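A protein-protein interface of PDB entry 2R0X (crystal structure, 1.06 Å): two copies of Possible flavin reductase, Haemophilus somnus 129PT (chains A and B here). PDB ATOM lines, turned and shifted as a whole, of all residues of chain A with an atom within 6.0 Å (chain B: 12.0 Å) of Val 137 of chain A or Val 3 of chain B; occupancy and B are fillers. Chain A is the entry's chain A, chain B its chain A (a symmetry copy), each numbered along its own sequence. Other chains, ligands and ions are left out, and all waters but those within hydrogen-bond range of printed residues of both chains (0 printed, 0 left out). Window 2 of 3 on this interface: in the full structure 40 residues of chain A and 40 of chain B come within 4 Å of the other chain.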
ATOM      1  N   PRO A  45     -26.022 -14.931  16.720  1.00  0.00           N
ATOM      2  CA  PRO A  45     -24.678 -14.414  16.480  1.00  0.00           C
ATOM      3  C   PRO A  45     -24.747 -12.908  16.247  1.00  0.00           C
ATOM      4  O   PRO A  45     -25.807 -12.367  16.116  1.00  0.00           O
ATOM      5  CB  PRO A  45     -24.298 -15.129  15.202  1.00  0.00           C
ATOM      6  CG  PRO A  45     -25.563 -15.213  14.454  1.00  0.00           C
ATOM      7  CD  PRO A  45     -26.621 -15.405  15.466  1.00  0.00           C
ATOM      8  N   PRO A  46     -23.586 -12.244  16.196  1.00  0.00           N
ATOM      9  CA  PRO A  46     -23.574 -10.829  15.900  1.00  0.00           C
ATOM     10  C   PRO A  46     -24.388 -10.493  14.657  1.00  0.00           C
ATOM     11  O   PRO A  46     -24.172 -11.041  13.572  1.00  0.00           O
ATOM     12  CB  PRO A  46     -22.080 -10.534  15.726  1.00  0.00           C
ATOM     13  CG  PRO A  46     -21.439 -11.452  16.700  1.00  0.00           C
ATOM     14  CD  PRO A  46     -22.223 -12.732  16.514  1.00  0.00           C
ATOM     15  N   THR A 103     -15.418 -10.363   2.762  1.00  0.00           N
ATOM     16  CA  THR A 103     -15.898 -11.697   2.477  1.00  0.00           C
ATOM     17  C   THR A 103     -17.015 -11.766   1.433  1.00  0.00           C
ATOM     18  O   THR A 103     -17.006 -12.657   0.562  1.00  0.00           O
ATOM     19  CB  THR A 103     -16.326 -12.398   3.795  1.00  0.00           C
ATOM     20  OG1 THR A 103     -15.214 -12.507   4.707  1.00  0.00           O
ATOM     21  CG2 THR A 103     -16.787 -13.807   3.466  1.00  0.00           C
ATOM     22  N   THR A 104     -17.985 -10.862   1.511  1.00  0.00           N
ATOM     23  CA  THR A 104     -19.168 -10.967   0.648  1.00  0.00           C
ATOM     24  C   THR A 104     -19.015 -10.414  -0.760  1.00  0.00           C
ATOM     25  O   THR A 104     -19.848 -10.670  -1.606  1.00  0.00           O
ATOM     26  CB  THR A 104     -20.389 -10.330   1.269  1.00  0.00           C
ATOM     27  OG1 THR A 104     -20.252  -8.917   1.220  1.00  0.00           O
ATOM     28  CG2 THR A 104     -20.692 -10.846   2.674  1.00  0.00           C
ATOM     29  N   ASP A 117     -19.248  -6.528   7.392  1.00  0.00           N
ATOM     30  CA  ASP A 117     -19.660  -7.259   6.173  1.00  0.00           C
ATOM     31  C   ASP A 117     -20.687  -8.303   6.577  1.00  0.00           C
ATOM     32  O   ASP A 117     -20.451  -9.018   7.520  1.00  0.00           O
ATOM     33  CB  ASP A 117     -18.425  -7.933   5.539  1.00  0.00           C
ATOM     34  CG  ASP A 117     -18.631  -8.232   4.068  1.00  0.00           C
ATOM     35  OD1 ASP A 117     -19.667  -7.834   3.513  1.00  0.00           O
ATOM     36  OD2 ASP A 117     -17.720  -8.862   3.477  1.00  0.00           O
ATOM     37  N   CYS A 118     -21.812  -8.305   5.874  1.00  0.00           N
ATOM     38  CA  CYS A 118     -22.998  -9.012   6.324  1.00  0.00           C
ATOM     39  C   CYS A 118     -23.705  -9.793   5.240  1.00  0.00           C
ATOM     40  O   CYS A 118     -23.687  -9.482   4.065  1.00  0.00           O
ATOM     41  CB  CYS A 118     -24.014  -8.004   6.871  1.00  0.00           C
ATOM     42  SG  CYS A 118     -23.451  -6.881   8.170  1.00  0.00           S
ATOM     43  N   GLU A 119     -24.376 -10.836   5.732  1.00  0.00           N
ATOM     44  CA  GLU A 119     -25.358 -11.569   4.954  1.00  0.00           C
ATOM     45  C   GLU A 119     -26.744 -11.107   5.350  1.00  0.00           C
ATOM     46  O   GLU A 119     -27.028 -10.979   6.537  1.00  0.00           O
ATOM     47  CB  GLU A 119     -25.235 -13.081   5.223  1.00  0.00           C
ATOM     48  CG  GLU A 119     -23.931 -13.666   4.664  1.00  0.00           C
ATOM     49  CD  GLU A 119     -23.612 -15.072   5.099  1.00  0.00           C
ATOM     50  OE1 GLU A 119     -24.301 -15.645   5.978  1.00  0.00           O
ATOM     51  OE2 GLU A 119     -22.591 -15.581   4.570  1.00  0.00           O
ATOM     52  N   LYS A 135     -26.688 -10.827   9.408  1.00  0.00           N
ATOM     53  CA  LYS A 135     -25.695 -11.563  10.154  1.00  0.00           C
ATOM     54  C   LYS A 135     -24.319 -11.040   9.747  1.00  0.00           C
ATOM     55  O   LYS A 135     -23.983 -11.019   8.569  1.00  0.00           O
ATOM     56  CB  LYS A 135     -25.796 -13.054   9.842  1.00  0.00           C
ATOM     57  CG  LYS A 135     -24.768 -13.863  10.569  1.00  0.00           C
ATOM     58  CD  LYS A 135     -24.774 -15.346  10.097  1.00  0.00           C
ATOM     59  CE  LYS A 135     -23.665 -16.104  10.688  1.00  0.00           C
ATOM     60  NZ  LYS A 135     -23.788 -17.506  10.162  1.00  0.00           N
ATOM     61  N   ILE A 136     -23.503 -10.688  10.713  1.00  0.00           N
ATOM     62  CA  ILE A 136     -22.151 -10.158  10.457  1.00  0.00           C
ATOM     63  C   ILE A 136     -21.191 -11.312  10.227  1.00  0.00           C
ATOM     64  O   ILE A 136     -21.084 -12.215  11.046  1.00  0.00           O
ATOM     65  CB  ILE A 136     -21.656  -9.265  11.606  1.00  0.00           C
ATOM     66  CG1 ILE A 136     -22.636  -8.080  11.782  1.00  0.00           C
ATOM     67  CG2 ILE A 136     -20.244  -8.799  11.361  1.00  0.00           C
ATOM     68  CD1 ILE A 136     -22.510  -7.452  13.128  1.00  0.00           C
ATOM     69  N   VAL A 137     -20.506 -11.300   9.093  1.00  0.00           N
ATOM     70  CA  VAL A 137     -19.570 -12.367   8.754  1.00  0.00           C
ATOM     71  C   VAL A 137     -18.116 -11.905   8.685  1.00  0.00           C
ATOM     72  O   VAL A 137     -17.239 -12.765   8.642  1.00  0.00           O
ATOM     73  CB  VAL A 137     -19.970 -13.116   7.482  1.00  0.00           C
ATOM     74  CG1 VAL A 137     -21.357 -13.785   7.684  1.00  0.00           C
ATOM     75  CG2 VAL A 137     -19.986 -12.197   6.268  1.00  0.00           C
ATOM     76  N   ASP A 138     -17.834 -10.595   8.724  1.00  0.00           N
ATOM     77  CA  ASP A 138     -16.463 -10.117   8.777  1.00  0.00           C
ATOM     78  C   ASP A 138     -16.539  -8.672   9.293  1.00  0.00           C
ATOM     79  O   ASP A 138     -17.516  -7.993   9.065  1.00  0.00           O
ATOM     80  CB  ASP A 138     -15.807 -10.232   7.363  1.00  0.00           C
ATOM     81  CG  ASP A 138     -14.324 -10.353   7.374  1.00  0.00           C
ATOM     82  OD1 ASP A 138     -13.685 -10.062   8.410  1.00  0.00           O
ATOM     83  OD2 ASP A 138     -13.790 -10.726   6.285  1.00  0.00           O
ATOM     84  N   ILE A 139     -15.506  -8.242  10.002  1.00  0.00           N
ATOM     85  CA  ILE A 139     -15.459  -6.899  10.600  1.00  0.00           C
ATOM     86  C   ILE A 139     -14.055  -6.369  10.403  1.00  0.00           C
ATOM     87  O   ILE A 139     -13.080  -7.084  10.566  1.00  0.00           O
ATOM     88  CB  ILE A 139     -15.792  -6.906  12.097  1.00  0.00           C
ATOM     89  CG1 ILE A 139     -17.248  -7.272  12.349  1.00  0.00           C
ATOM     90  CG2 ILE A 139     -15.447  -5.560  12.779  1.00  0.00           C
ATOM     91  CD1 ILE A 139     -17.685  -7.305  13.826  1.00  0.00           C
ATOM     92  N   VAL B   3     -18.610 -13.905  13.131  1.00  0.00           N
ATOM     93  CA  VAL B   3     -17.482 -13.206  13.823  1.00  0.00           C
ATOM     94  C   VAL B   3     -17.537 -13.492  15.316  1.00  0.00           C
ATOM     95  O   VAL B   3     -18.583 -13.915  15.827  1.00  0.00           O
ATOM     96  CB  VAL B   3     -17.543 -11.684  13.554  1.00  0.00           C
ATOM     97  CG1 VAL B   3     -17.409 -11.412  12.069  1.00  0.00           C
ATOM     98  CG2 VAL B   3     -18.849 -11.085  14.093  1.00  0.00           C
ATOM     99  N   GLU B   4     -16.429 -13.258  16.024  1.00  0.00           N
ATOM    100  CA  GLU B   4     -16.394 -13.489  17.467  1.00  0.00           C
ATOM    101  C   GLU B   4     -17.187 -12.418  18.195  1.00  0.00           C
ATOM    102  O   GLU B   4     -17.224 -11.238  17.787  1.00  0.00           O
ATOM    103  CB  GLU B   4     -14.960 -13.501  18.000  1.00  0.00           C
ATOM    104  CG  GLU B   4     -14.109 -14.659  17.513  1.00  0.00           C
ATOM    105  N   VAL B   5     -17.809 -12.803  19.286  1.00  0.00           N
ATOM    106  CA  VAL B   5     -18.614 -11.854  20.032  1.00  0.00           C
ATOM    107  C   VAL B   5     -17.759 -10.700  20.557  1.00  0.00           C
ATOM    108  O   VAL B   5     -18.189  -9.544  20.526  1.00  0.00           O
ATOM    109  CB  VAL B   5     -19.413 -12.549  21.169  1.00  0.00           C
ATOM    110  CG1 VAL B   5     -20.126 -11.517  22.036  1.00  0.00           C
ATOM    111  CG2 VAL B   5     -20.429 -13.545  20.583  1.00  0.00           C
ATOM    112  N   SER B   6     -16.567 -10.984  21.069  1.00  0.00           N
ATOM    113  CA  SER B   6     -15.727  -9.911  21.628  1.00  0.00           C
ATOM    114  C   SER B   6     -15.360  -8.870  20.568  1.00  0.00           C
ATOM    115  O   SER B   6     -15.363  -7.664  20.841  1.00  0.00           O
ATOM    116  CB  SER B   6     -14.437 -10.507  22.214  1.00  0.00           C
ATOM    117  OG  SER B   6     -13.807 -11.293  21.212  1.00  0.00           O
ATOM    118  N   GLN B   7     -15.044  -9.344  19.367  1.00  0.00           N
ATOM    119  CA  GLN B   7     -14.724  -8.454  18.259  1.00  0.00           C
ATOM    120  C   GLN B   7     -15.927  -7.602  17.863  1.00  0.00           C
ATOM    121  O   GLN B   7     -15.774  -6.430  17.577  1.00  0.00           O
ATOM    122  CB  GLN B   7     -14.211  -9.241  17.058  1.00  0.00           C
ATOM    123  CG  GLN B   7     -14.012  -8.404  15.813  1.00  0.00           C
ATOM    124  N   PHE B   8     -17.105  -8.215  17.843  1.00  0.00           N
ATOM    125  CA  PHE B   8     -18.304  -7.464  17.556  1.00  0.00           C
ATOM    126  C   PHE B   8     -18.560  -6.403  18.614  1.00  0.00           C
ATOM    127  O   PHE B   8     -18.878  -5.265  18.260  1.00  0.00           O
ATOM    128  CB  PHE B   8     -19.487  -8.415  17.538  1.00  0.00           C
ATOM    129  CG  PHE B   8     -20.824  -7.758  17.353  1.00  0.00           C
ATOM    130  CD1 PHE B   8     -21.063  -6.960  16.263  1.00  0.00           C
ATOM    131  CD2 PHE B   8     -21.845  -7.951  18.258  1.00  0.00           C
ATOM    132  CE1 PHE B   8     -22.305  -6.376  16.057  1.00  0.00           C
ATOM    133  CE2 PHE B   8     -23.091  -7.353  18.043  1.00  0.00           C
ATOM    134  CZ  PHE B   8     -23.310  -6.574  16.959  1.00  0.00           C
ATOM    135  N   LYS B   9     -18.409  -6.762  19.896  1.00  0.00           N
ATOM    136  CA  LYS B   9     -18.641  -5.767  20.969  1.00  0.00           C
ATOM    137  C   LYS B   9     -17.663  -4.598  20.860  1.00  0.00           C
ATOM    138  O   LYS B   9     -18.043  -3.448  21.052  1.00  0.00           O
ATOM    139  CB  LYS B   9     -18.607  -6.407  22.373  1.00  0.00           C
ATOM    140  CG  LYS B   9     -19.750  -7.400  22.613  1.00  0.00           C
ATOM    141  CD  LYS B   9     -19.653  -8.083  23.949  1.00  0.00           C
ATOM    142  N   ASP B  10     -16.408  -4.883  20.540  1.00  0.00           N
ATOM    143  CA  ASP B  10     -15.440  -3.809  20.416  1.00  0.00           C
ATOM    144  C   ASP B  10     -15.739  -2.950  19.214  1.00  0.00           C
ATOM    145  O   ASP B  10     -15.556  -1.739  19.288  1.00  0.00           O
ATOM    146  CB  ASP B  10     -14.044  -4.375  20.319  1.00  0.00           C
ATOM    147  CG  ASP B  10     -13.541  -4.910  21.643  1.00  0.00           C
ATOM    148  OD1 ASP B  10     -14.101  -4.579  22.720  1.00  0.00           O
ATOM    149  OD2 ASP B  10     -12.595  -5.700  21.609  1.00  0.00           O
ATOM    150  N   ALA B  11     -16.156  -3.560  18.111  1.00  0.00           N
ATOM    151  CA  ALA B  11     -16.574  -2.774  16.924  1.00  0.00           C
ATOM    152  C   ALA B  11     -17.788  -1.925  17.252  1.00  0.00           C
ATOM    153  O   ALA B  11     -17.825  -0.747  16.941  1.00  0.00           O
ATOM    154  CB  ALA B  11     -16.832  -3.638  15.687  1.00  0.00           C
ATOM    155  N   MET B  12     -18.772  -2.494  17.949  1.00  0.00           N
ATOM    156  CA  MET B  12     -19.967  -1.721  18.331  1.00  0.00           C
ATOM    157  C   MET B  12     -19.634  -0.565  19.256  1.00  0.00           C
ATOM    158  O   MET B  12     -20.277   0.495  19.187  1.00  0.00           O
ATOM    159  CB  MET B  12     -21.031  -2.587  18.990  1.00  0.00           C
ATOM    160  CG  MET B  12     -21.754  -3.535  18.021  1.00  0.00           C
ATOM    161  SD  MET B  12     -22.591  -2.552  16.540  1.00  0.00           S
ATOM    162  CE  MET B  12     -23.786  -1.419  17.555  1.00  0.00           C
ATOM    163  N   ALA B  13     -18.627  -0.737  20.100  1.00  0.00           N
ATOM    164  CA  ALA B  13     -18.189   0.365  20.980  1.00  0.00           C
ATOM    165  C   ALA B  13     -17.785   1.611  20.189  1.00  0.00           C
ATOM    166  O   ALA B  13     -17.842   2.730  20.702  1.00  0.00           O
ATOM    167  CB  ALA B  13     -17.061  -0.078  21.890  1.00  0.00           C
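The backbone carbonyl oxygen (O) of Pro 46 of chain A lies within hydrogen-bond range of the backbone NH (N) of Ile 136 of chain A (3.0 Å). OD2 of Asp 138 of chain A is in hydrogen-bond range of OG1 of Thr 103 of chain A (2.8 Å). The backbone carbonyl oxygen (O) of Asp 117 of chain A lies within hydrogen-bond range of the backbone NH (N) of Val 137 of chain A (2.8 Å). N of Asp 117 of chain A lies within hydrogen-bond range of O of Asp 138 of chain A, 2.8 Å away.
Among the printed residues, pairs that only touch across the chains: Ile 136 of chain A with Phe 8 of chain B, Pro 46 of chain A with Phe 8 of chain B, Asp 138 of chain A with Val 3 of chain B, Val 137 of chain A with Val 3 of chain B, Ile 136 of chain A with Val 3 of chain B, Pro 46 of chain A with Val 3 of chain B, Ile 139 of chain A with Ala 11 of chain B, Ile 139 of chain A with Phe 8 of chain B and Ile 139 of chain A with Val 3 of chain B.
Of the printed residues of chain B, Pro 46 of chain A touches Val 3 (3.7 Å) and Phe 8 (3.5 Å). No residue of chain B comes within 4 Å of Asp 117 of chain A. No residue of chain B comes within 4 Å of Cys 118 of chain A. No residue of chain B comes within 4 Å of Glu 119 of chain A. No residue of chain B comes within 4 Å of Lys 135 of chain A. Ile 136 of chain A touches just these residues of chain B: Val 3 (3.7 Å) and Phe 8 (3.1 Å). Val 137 of chain A touches one residue of chain B. Printed residues of chain B within 4 Å of Ile 139 of chain A: Val 3, Phe 8 and Ala 11. Val 3 of chain B touches five residues of chain A. Val 5 of chain B touches none of the printed residues of chain A. Gln 7 of chain B touches none of the printed residues of chain A. Printed residues of chain A within 4 Å of Phe 8 of chain B: Pro 46, Ile 136 and Ile 139. Of the printed residues of chain A, Ala 11 of chain B touches Ile 139. The nearest residue of chain B that does not touch Val 137 of chain A is Glu 4 of chain B (7.4 Å). The nearest residue of chain A that does not touch Val 3 of chain B is Pro 45 of chain A (5.9 Å).
Of the 11 printed residues of chain B, 3 touch a printed residue of chain A. Printed residues of chain B that touch a printed residue of chain A: Val 3, Phe 8 and Ala 11. Hydrophobic or aromatic side chains of chain B within 4 Å of the printed part of chain A: Val 3, Phe 8 and Ala 11. Hydrophobic or aromatic side chains of chain A that line the printed part of chain B: Pro 46, Ile 136 and Ile 139. Among the printed residues, no Asp or Glu carboxylate lies within 4 Å of a Lys or Arg side-chain nitrogen of the other chain.
No position is printed for both chains. Of the 9 pairs that touch across the chains among the printed residues, none has its exchanged pair printed and touching as well.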
